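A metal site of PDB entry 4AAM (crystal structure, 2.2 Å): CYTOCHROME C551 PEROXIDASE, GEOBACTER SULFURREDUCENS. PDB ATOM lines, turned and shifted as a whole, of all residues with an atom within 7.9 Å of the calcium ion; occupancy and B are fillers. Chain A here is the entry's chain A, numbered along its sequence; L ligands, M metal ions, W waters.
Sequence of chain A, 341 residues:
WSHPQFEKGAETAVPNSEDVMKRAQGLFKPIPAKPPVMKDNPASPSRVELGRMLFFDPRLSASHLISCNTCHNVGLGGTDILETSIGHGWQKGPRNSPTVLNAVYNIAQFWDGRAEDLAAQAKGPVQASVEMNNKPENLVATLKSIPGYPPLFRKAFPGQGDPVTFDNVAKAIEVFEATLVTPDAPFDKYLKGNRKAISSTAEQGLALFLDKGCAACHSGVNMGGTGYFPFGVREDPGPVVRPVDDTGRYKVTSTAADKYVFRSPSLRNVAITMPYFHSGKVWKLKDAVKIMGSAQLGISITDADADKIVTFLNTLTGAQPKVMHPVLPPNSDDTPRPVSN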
ATOM      1  N   THR A  79     -19.325   1.979  -2.941  1.00  0.00           N
ATOM      2  CA  THR A  79     -19.639   0.625  -3.398  1.00  0.00           C
ATOM      3  C   THR A  79     -18.791   0.285  -4.613  1.00  0.00           C
ATOM      4  O   THR A  79     -17.964   1.103  -5.036  1.00  0.00           O
ATOM      5  CB  THR A  79     -21.165   0.453  -3.768  1.00  0.00           C
ATOM      6  OG1 THR A  79     -21.539   1.375  -4.824  1.00  0.00           O
ATOM      7  CG2 THR A  79     -22.056   0.716  -2.569  1.00  0.00           C
ATOM      8  N   ASP A  80     -19.015  -0.891  -5.201  1.00  0.00           N
ATOM      9  CA  ASP A  80     -18.325  -1.282  -6.405  1.00  0.00           C
ATOM     10  C   ASP A  80     -19.179  -1.372  -7.690  1.00  0.00           C
ATOM     11  O   ASP A  80     -18.653  -1.776  -8.711  1.00  0.00           O
ATOM     12  CB  ASP A  80     -17.526  -2.583  -6.183  1.00  0.00           C
ATOM     13  CG  ASP A  80     -18.424  -3.818  -5.896  1.00  0.00           C
ATOM     14  OD1 ASP A  80     -19.669  -3.760  -6.076  1.00  0.00           O
ATOM     15  OD2 ASP A  80     -17.850  -4.887  -5.523  1.00  0.00           O
ATOM     16  N   ILE A  81     -20.469  -0.984  -7.653  1.00  0.00           N
ATOM     17  CA  ILE A  81     -21.401  -1.132  -8.819  1.00  0.00           C
ATOM     18  C   ILE A  81     -21.371  -2.447  -9.588  1.00  0.00           C
ATOM     19  O   ILE A  81     -21.594  -2.491 -10.802  1.00  0.00           O
ATOM     20  CB  ILE A  81     -21.338   0.082  -9.787  1.00  0.00           C
ATOM     21  CG1 ILE A  81     -19.907   0.248 -10.353  1.00  0.00           C
ATOM     22  CG2 ILE A  81     -21.890   1.326  -9.061  1.00  0.00           C
ATOM     23  CD1 ILE A  81     -19.719   1.421 -11.310  1.00  0.00           C
ATOM     24  N   LEU A  82     -21.089  -3.529  -8.862  1.00  0.00           N
ATOM     25  CA  LEU A  82     -21.210  -4.868  -9.447  1.00  0.00           C
ATOM     26  C   LEU A  82     -22.316  -5.606  -8.730  1.00  0.00           C
ATOM     27  O   LEU A  82     -22.630  -5.302  -7.565  1.00  0.00           O
ATOM     28  CB  LEU A  82     -19.931  -5.664  -9.217  1.00  0.00           C
ATOM     29  CG  LEU A  82     -18.610  -5.019  -9.716  1.00  0.00           C
ATOM     30  CD1 LEU A  82     -17.496  -5.975  -9.366  1.00  0.00           C
ATOM     31  CD2 LEU A  82     -18.701  -4.800 -11.222  1.00  0.00           C
ATOM     32  N   GLU A  83     -22.839  -6.663  -9.384  1.00  0.00           N
ATOM     33  CA  GLU A  83     -23.814  -7.538  -8.777  1.00  0.00           C
ATOM     34  C   GLU A  83     -23.325  -8.064  -7.438  1.00  0.00           C
ATOM     35  O   GLU A  83     -23.991  -7.848  -6.407  1.00  0.00           O
ATOM     36  CB  GLU A  83     -24.181  -8.694  -9.748  1.00  0.00           C
ATOM     37  CG  GLU A  83     -25.024  -8.143 -10.867  1.00  0.00           C
ATOM     38  CD  GLU A  83     -25.692  -9.176 -11.730  1.00  0.00           C
ATOM     39  OE1 GLU A  83     -25.561 -10.395 -11.487  1.00  0.00           O
ATOM     40  OE2 GLU A  83     -26.419  -8.755 -12.636  1.00  0.00           O
ATOM     41  N   ASN A  96     -23.833  -8.632  -2.808  1.00  0.00           N
ATOM     42  CA  ASN A  96     -23.585  -7.274  -3.226  1.00  0.00           C
ATOM     43  C   ASN A  96     -22.871  -6.495  -2.119  1.00  0.00           C
ATOM     44  O   ASN A  96     -23.201  -6.636  -0.949  1.00  0.00           O
ATOM     45  CB  ASN A  96     -24.913  -6.596  -3.604  1.00  0.00           C
ATOM     46  CG  ASN A  96     -24.709  -5.228  -4.236  1.00  0.00           C
ATOM     47  OD1 ASN A  96     -24.961  -4.204  -3.578  1.00  0.00           O
ATOM     48  ND2 ASN A  96     -24.255  -5.177  -5.496  1.00  0.00           N
ATOM     49  N   SER A  97     -21.890  -5.683  -2.511  1.00  0.00           N
ATOM     50  CA  SER A  97     -21.140  -4.870  -1.568  1.00  0.00           C
ATOM     51  C   SER A  97     -21.960  -3.635  -1.188  1.00  0.00           C
ATOM     52  O   SER A  97     -22.294  -2.824  -2.043  1.00  0.00           O
ATOM     53  CB  SER A  97     -19.789  -4.463  -2.182  1.00  0.00           C
ATOM     54  OG  SER A  97     -19.315  -3.254  -1.627  1.00  0.00           O
ATOM     55  N   PRO A  98     -22.324  -3.526   0.091  1.00  0.00           N
ATOM     56  CA  PRO A  98     -23.071  -2.367   0.595  1.00  0.00           C
ATOM     57  C   PRO A  98     -22.151  -1.185   0.865  1.00  0.00           C
ATOM     58  O   PRO A  98     -20.910  -1.338   1.013  1.00  0.00           O
ATOM     59  CB  PRO A  98     -23.638  -2.863   1.938  1.00  0.00           C
ATOM     60  CG  PRO A  98     -22.619  -3.835   2.408  1.00  0.00           C
ATOM     61  CD  PRO A  98     -22.050  -4.500   1.185  1.00  0.00           C
ATOM     62  N   THR A  99     -22.732   0.004   0.949  1.00  0.00           N
ATOM     63  CA  THR A  99     -21.888   1.213   1.055  1.00  0.00           C
ATOM     64  C   THR A  99     -21.294   1.352   2.443  1.00  0.00           C
ATOM     65  O   THR A  99     -21.986   1.117   3.435  1.00  0.00           O
ATOM     66  CB  THR A  99     -22.697   2.480   0.717  1.00  0.00           C
ATOM     67  OG1 THR A  99     -21.806   3.587   0.712  1.00  0.00           O
ATOM     68  CG2 THR A  99     -23.818   2.757   1.715  1.00  0.00           C
ATOM     69  N   TRP A 111     -24.928  -7.878   5.689  1.00  0.00           N
ATOM     70  CA  TRP A 111     -26.342  -8.068   5.358  1.00  0.00           C
ATOM     71  C   TRP A 111     -27.032  -8.909   6.393  1.00  0.00           C
ATOM     72  O   TRP A 111     -28.284  -8.869   6.548  1.00  0.00           O
ATOM     73  CB  TRP A 111     -26.476  -8.759   4.016  1.00  0.00           C
ATOM     74  CG  TRP A 111     -26.289  -7.836   2.860  1.00  0.00           C
ATOM     75  CD1 TRP A 111     -25.129  -7.650   2.081  1.00  0.00           C
ATOM     76  CD2 TRP A 111     -27.287  -6.959   2.296  1.00  0.00           C
ATOM     77  NE1 TRP A 111     -25.376  -6.737   1.070  1.00  0.00           N
ATOM     78  CE2 TRP A 111     -26.654  -6.279   1.150  1.00  0.00           C
ATOM     79  CE3 TRP A 111     -28.639  -6.703   2.573  1.00  0.00           C
ATOM     80  CZ2 TRP A 111     -27.333  -5.405   0.368  1.00  0.00           C
ATOM     81  CZ3 TRP A 111     -29.313  -5.780   1.770  1.00  0.00           C
ATOM     82  CH2 TRP A 111     -28.670  -5.156   0.695  1.00  0.00           C
ATOM     83  N   ASN A 269     -28.230   7.380   0.073  1.00  0.00           N
ATOM     84  CA  ASN A 269     -27.433   7.291  -1.130  1.00  0.00           C
ATOM     85  C   ASN A 269     -27.886   6.111  -1.988  1.00  0.00           C
ATOM     86  O   ASN A 269     -27.132   5.688  -2.856  1.00  0.00           O
ATOM     87  CB  ASN A 269     -25.981   7.210  -0.751  1.00  0.00           C
ATOM     88  CG  ASN A 269     -25.546   8.412   0.077  1.00  0.00           C
ATOM     89  OD1 ASN A 269     -25.586   9.528  -0.435  1.00  0.00           O
ATOM     90  ND2 ASN A 269     -25.118   8.193   1.358  1.00  0.00           N
ATOM     91  N   VAL A 270     -29.111   5.607  -1.793  1.00  0.00           N
ATOM     92  CA  VAL A 270     -29.534   4.423  -2.549  1.00  0.00           C
ATOM     93  C   VAL A 270     -29.545   4.671  -4.090  1.00  0.00           C
ATOM     94  O   VAL A 270     -29.276   3.750  -4.864  1.00  0.00           O
ATOM     95  CB  VAL A 270     -30.913   3.885  -2.111  1.00  0.00           C
ATOM     96  CG1 VAL A 270     -31.998   4.916  -2.498  1.00  0.00           C
ATOM     97  CG2 VAL A 270     -31.192   2.520  -2.725  1.00  0.00           C
ATOM     98  N   ILE A 272     -27.302   5.978  -5.904  1.00  0.00           N
ATOM     99  CA  ILE A 272     -26.000   5.796  -6.547  1.00  0.00           C
ATOM    100  C   ILE A 272     -25.290   4.478  -6.173  1.00  0.00           C
ATOM    101  O   ILE A 272     -24.062   4.326  -6.402  1.00  0.00           O
ATOM    102  CB  ILE A 272     -25.063   6.987  -6.308  1.00  0.00           C
ATOM    103  CG1 ILE A 272     -24.600   6.977  -4.839  1.00  0.00           C
ATOM    104  CG2 ILE A 272     -25.755   8.324  -6.709  1.00  0.00           C
ATOM    105  CD1 ILE A 272     -23.711   8.154  -4.456  1.00  0.00           C
ATOM    106  N   THR A 273     -26.048   3.545  -5.578  1.00  0.00           N
ATOM    107  CA  THR A 273     -25.397   2.333  -5.071  1.00  0.00           C
ATOM    108  C   THR A 273     -26.033   1.117  -5.743  1.00  0.00           C
ATOM    109  O   THR A 273     -26.060   0.060  -5.147  1.00  0.00           O
ATOM    110  CB  THR A 273     -25.400   2.193  -3.507  1.00  0.00           C
ATOM    111  OG1 THR A 273     -26.759   2.151  -3.034  1.00  0.00           O
ATOM    112  CG2 THR A 273     -24.716   3.360  -2.821  1.00  0.00           C
ATOM    113  N   MET A 274     -26.558   1.288  -6.962  1.00  0.00           N
ATOM    114  CA  MET A 274     -27.066   0.136  -7.742  1.00  0.00           C
ATOM    115  C   MET A 274     -25.976  -0.913  -7.990  1.00  0.00           C
ATOM    116  O   MET A 274     -24.823  -0.578  -7.929  1.00  0.00           O
ATOM    117  CB  MET A 274     -27.699   0.611  -9.067  1.00  0.00           C
ATOM    118  CG  MET A 274     -26.725   1.145 -10.073  1.00  0.00           C
ATOM    119  SD  MET A 274     -26.092   2.746  -9.634  1.00  0.00           S
ATOM    120  CE  MET A 274     -27.431   3.780 -10.249  1.00  0.00           C
ATOM    121  N   PRO A 275     -26.320  -2.191  -8.199  1.00  0.00           N
ATOM    122  CA  PRO A 275     -27.610  -2.802  -8.114  1.00  0.00           C
ATOM    123  C   PRO A 275     -27.999  -3.058  -6.627  1.00  0.00           C
ATOM    124  O   PRO A 275     -27.222  -2.727  -5.669  1.00  0.00           O
ATOM    125  CB  PRO A 275     -27.434  -4.108  -8.927  1.00  0.00           C
ATOM    126  CG  PRO A 275     -26.003  -4.486  -8.666  1.00  0.00           C
ATOM    127  CD  PRO A 275     -25.264  -3.154  -8.600  1.00  0.00           C
ATOM    128  N   TYR A 276     -29.156  -3.652  -6.455  1.00  0.00           N
ATOM    129  CA  TYR A 276     -29.891  -3.623  -5.236  1.00  0.00           C
ATOM    130  C   TYR A 276     -30.195  -5.024  -4.717  1.00  0.00           C
ATOM    131  O   TYR A 276     -30.165  -6.020  -5.491  1.00  0.00           O
ATOM    132  CB  TYR A 276     -31.175  -2.842  -5.457  1.00  0.00           C
ATOM    133  CG  TYR A 276     -30.850  -1.421  -5.884  1.00  0.00           C
ATOM    134  CD1 TYR A 276     -30.235  -0.538  -5.008  1.00  0.00           C
ATOM    135  CD2 TYR A 276     -31.156  -0.980  -7.177  1.00  0.00           C
ATOM    136  CE1 TYR A 276     -29.920   0.759  -5.379  1.00  0.00           C
ATOM    137  CE2 TYR A 276     -30.882   0.348  -7.573  1.00  0.00           C
ATOM    138  CZ  TYR A 276     -30.249   1.200  -6.671  1.00  0.00           C
ATOM    139  OH  TYR A 276     -29.988   2.478  -7.041  1.00  0.00           O
ATOM    140  N   PHE A 277     -30.504  -5.053  -3.410  1.00  0.00           N
ATOM    141  CA  PHE A 277     -30.633  -6.310  -2.648  1.00  0.00           C
ATOM    142  C   PHE A 277     -29.296  -6.992  -2.385  1.00  0.00           C
ATOM    143  O   PHE A 277     -28.294  -6.618  -2.983  1.00  0.00           O
ATOM    144  CB  PHE A 277     -31.742  -7.241  -3.263  1.00  0.00           C
ATOM    145  CG  PHE A 277     -33.048  -6.492  -3.447  1.00  0.00           C
ATOM    146  CD1 PHE A 277     -33.549  -5.677  -2.425  1.00  0.00           C
ATOM    147  CD2 PHE A 277     -33.722  -6.520  -4.654  1.00  0.00           C
ATOM    148  CE1 PHE A 277     -34.734  -4.947  -2.600  1.00  0.00           C
ATOM    149  CE2 PHE A 277     -34.899  -5.788  -4.834  1.00  0.00           C
ATOM    150  CZ  PHE A 277     -35.414  -5.017  -3.807  1.00  0.00           C
ATOM    151  N   HIS A 278     -29.282  -7.959  -1.467  1.00  0.00           N
ATOM    152  CA  HIS A 278     -28.029  -8.635  -1.058  1.00  0.00           C
ATOM    153  C   HIS A 278     -27.501  -9.450  -2.204  1.00  0.00           C
ATOM    154  O   HIS A 278     -26.327  -9.780  -2.275  1.00  0.00           O
ATOM    155  CB  HIS A 278     -28.297  -9.507   0.174  1.00  0.00           C
ATOM    156  CG  HIS A 278     -29.134 -10.716  -0.117  1.00  0.00           C
ATOM    157  ND1 HIS A 278     -30.491 -10.697  -0.043  1.00  0.00           N
ATOM    158  CD2 HIS A 278     -28.778 -11.992  -0.574  1.00  0.00           C
ATOM    159  CE1 HIS A 278     -30.972 -11.903  -0.389  1.00  0.00           C
ATOM    160  NE2 HIS A 278     -29.941 -12.696  -0.728  1.00  0.00           N
ATOM    161  N   GLY A 280     -27.781  -8.417  -5.404  1.00  0.00           N
ATOM    162  CA  GLY A 280     -27.295  -7.496  -6.463  1.00  0.00           C
ATOM    163  C   GLY A 280     -27.898  -7.812  -7.827  1.00  0.00           C
ATOM    164  O   GLY A 280     -27.360  -7.476  -8.851  1.00  0.00           O
ATOM    165  N   VAL A 282     -31.033  -6.800  -8.943  1.00  0.00           N
ATOM    166  CA  VAL A 282     -32.062  -5.867  -9.422  1.00  0.00           C
ATOM    167  C   VAL A 282     -31.339  -4.550  -9.653  1.00  0.00           C
ATOM    168  O   VAL A 282     -30.924  -3.887  -8.697  1.00  0.00           O
ATOM    169  CB  VAL A 282     -33.189  -5.701  -8.377  1.00  0.00           C
ATOM    170  CG1 VAL A 282     -34.232  -4.666  -8.811  1.00  0.00           C
ATOM    171  CG2 VAL A 282     -33.821  -7.059  -8.067  1.00  0.00           C
HETATM  172 FE1  LIG L   1     -37.219  -2.327   1.903  1.00  0.00          FE
HETATM  173  C1  LIG L   1     -34.265  -3.572   0.738  1.00  0.00           C
HETATM  174  C2  LIG L   1     -37.137   0.270  -0.405  1.00  0.00           C
HETATM  175  C3  LIG L   1     -40.610  -1.720   2.385  1.00  0.00           C
HETATM  176  C4  LIG L   1     -37.179  -4.418   4.603  1.00  0.00           C
HETATM  177  N1  LIG L   1     -35.917  -1.730   0.519  1.00  0.00           N
HETATM  178  C5  LIG L   1     -34.768  -2.406   0.132  1.00  0.00           C
HETATM  179  C6  LIG L   1     -34.153  -1.664  -0.945  1.00  0.00           C
HETATM  180  C7  LIG L   1     -34.971  -0.609  -1.246  1.00  0.00           C
HETATM  181  C8  LIG L   1     -36.096  -0.660  -0.341  1.00  0.00           C
HETATM  182  C9  LIG L   1     -34.750   0.464  -2.318  1.00  0.00           C
HETATM  183  C10 LIG L   1     -32.816  -1.958  -1.636  1.00  0.00           C
HETATM  184  C11 LIG L   1     -31.728  -1.049  -0.958  1.00  0.00           C
HETATM  185  C12 LIG L   1     -30.330  -1.651  -1.217  1.00  0.00           C
HETATM  186  O1  LIG L   1     -29.287  -1.097  -0.762  1.00  0.00           O
HETATM  187  O2  LIG L   1     -30.150  -2.748  -1.836  1.00  0.00           O
HETATM  188  N2  LIG L   1     -38.736  -0.801   1.072  1.00  0.00           N
HETATM  189  C13 LIG L   1     -38.423   0.068   0.126  1.00  0.00           C
HETATM  190  C14 LIG L   1     -39.605   0.760  -0.185  1.00  0.00           C
HETATM  191  C15 LIG L   1     -40.597   0.166   0.593  1.00  0.00           C
HETATM  192  C16 LIG L   1     -39.984  -0.870   1.425  1.00  0.00           C
HETATM  193  C17 LIG L   1     -39.677   1.858  -1.203  1.00  0.00           C
HETATM  194  C18 LIG L   1     -42.061   0.415   0.654  1.00  0.00           C
HETATM  195  C19 LIG L   1     -42.718   0.135  -0.498  1.00  0.00           C
HETATM  196  N3  LIG L   1     -38.629  -2.960   3.312  1.00  0.00           N
HETATM  197  C20 LIG L   1     -39.965  -2.563   3.329  1.00  0.00           C
HETATM  198  C21 LIG L   1     -40.585  -3.131   4.484  1.00  0.00           C
HETATM  199  C22 LIG L   1     -39.605  -3.917   5.128  1.00  0.00           C
HETATM  200  C23 LIG L   1     -38.393  -3.805   4.341  1.00  0.00           C
HETATM  201  C24 LIG L   1     -42.029  -2.896   4.866  1.00  0.00           C
HETATM  202  C25 LIG L   1     -39.697  -4.770   6.376  1.00  0.00           C
HETATM  203  C26 LIG L   1     -40.637  -5.751   6.514  1.00  0.00           C
HETATM  204  N4  LIG L   1     -35.994  -3.643   2.554  1.00  0.00           N
HETATM  205  C27 LIG L   1     -36.158  -4.482   3.643  1.00  0.00           C
HETATM  206  C28 LIG L   1     -35.067  -5.456   3.770  1.00  0.00           C
HETATM  207  C29 LIG L   1     -34.283  -5.201   2.675  1.00  0.00           C
HETATM  208  C30 LIG L   1     -34.873  -4.073   1.911  1.00  0.00           C
HETATM  209  C31 LIG L   1     -34.844  -6.535   4.867  1.00  0.00           C
HETATM  210  C32 LIG L   1     -33.024  -5.970   2.301  1.00  0.00           C
HETATM  211  C33 LIG L   1     -33.557  -7.204   1.516  1.00  0.00           C
HETATM  212  C34 LIG L   1     -32.448  -8.012   0.840  1.00  0.00           C
HETATM  213  O3  LIG L   1     -31.728  -7.529  -0.077  1.00  0.00           O
HETATM  214  O4  LIG L   1     -32.231  -9.202   1.237  1.00  0.00           O
HETATM  215 CA    CA M   1     -26.041  -2.023  -3.962  1.00  0.00          CA
HETATM  216  O   HOH W   1     -27.522  -3.485  -2.621  1.00  0.00           O
HETATM  217  O   HOH W   2     -24.572  -1.231  -2.421  1.00  0.00           O
HETATM  218  O   HOH W   3     -24.050  -2.111  -5.465  1.00  0.00           O
HETATM  219  O   HOH W   4     -27.507  -0.391  -2.774  1.00  0.00           O
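Within 4 Å of the calcium ion: Asn 96, Thr 273 and Pro 275.
The nearest printed residue that does not touch the calcium ion is Met 274 (4.2 Å).
The calcium ion is bound by the backbone carbonyl oxygen of Pro 275 (2.2 Å), water W2 (2.3 Å), the backbone carbonyl oxygen of Thr 273 (2.4 Å), the side-chain amide oxygen of Asn 96 (2.5 Å), water W1 (2.5 Å), water W4 (2.5 Å) and water W3 (2.5 Å).
The calcium ion has seven donor atoms within binding distance.
The backbone NH (N) of Phe 277 is in hydrogen-bond range of an oxygen (O2) of the ligand, at 2.8 Å.
An oxygen (O3) of the ligand is in hydrogen-bond range of the backbone NH of His 278, at 2.8 Å.
ND1 of His 278 is in hydrogen-bond range of O4 of the ligand (2.6 Å).
Water W1 lies within hydrogen-bond range of an oxygen (O2) of the ligand (2.8 Å) and the backbone carbonyl oxygen (O) of Phe 277 (3.2 Å).
Water W3 bridges the backbone carbonyl oxygen (O) of Met 274 (3.0 Å) and the side-chain amide nitrogen (ND2) of Asn 96 (3.1 Å).
Water W4 bridges the side-chain hydroxyl of Thr 273 (2.7 Å) and an oxygen (O1) of the ligand (2.8 Å).
The side-chain hydroxyl (OG1) of Thr 273 is in hydrogen-bond range of the backbone carbonyl oxygen (O) of Val 270, at 3.5 Å.
NE1 of Trp 111 sits at hydrogen-bond distance from O of Asn 96, 3.0 Å away.
The backbone carbonyl oxygen of Leu 82 lies within hydrogen-bond range of the side-chain amide nitrogen of Asn 96 (2.6 Å).
O of Glu 83 is in hydrogen-bond range of ND2 of Asn 96, at 2.8 Å.
The backbone NH (N) of Asn 96 sits at hydrogen-bond distance from the backbone carbonyl oxygen (O) of His 278.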
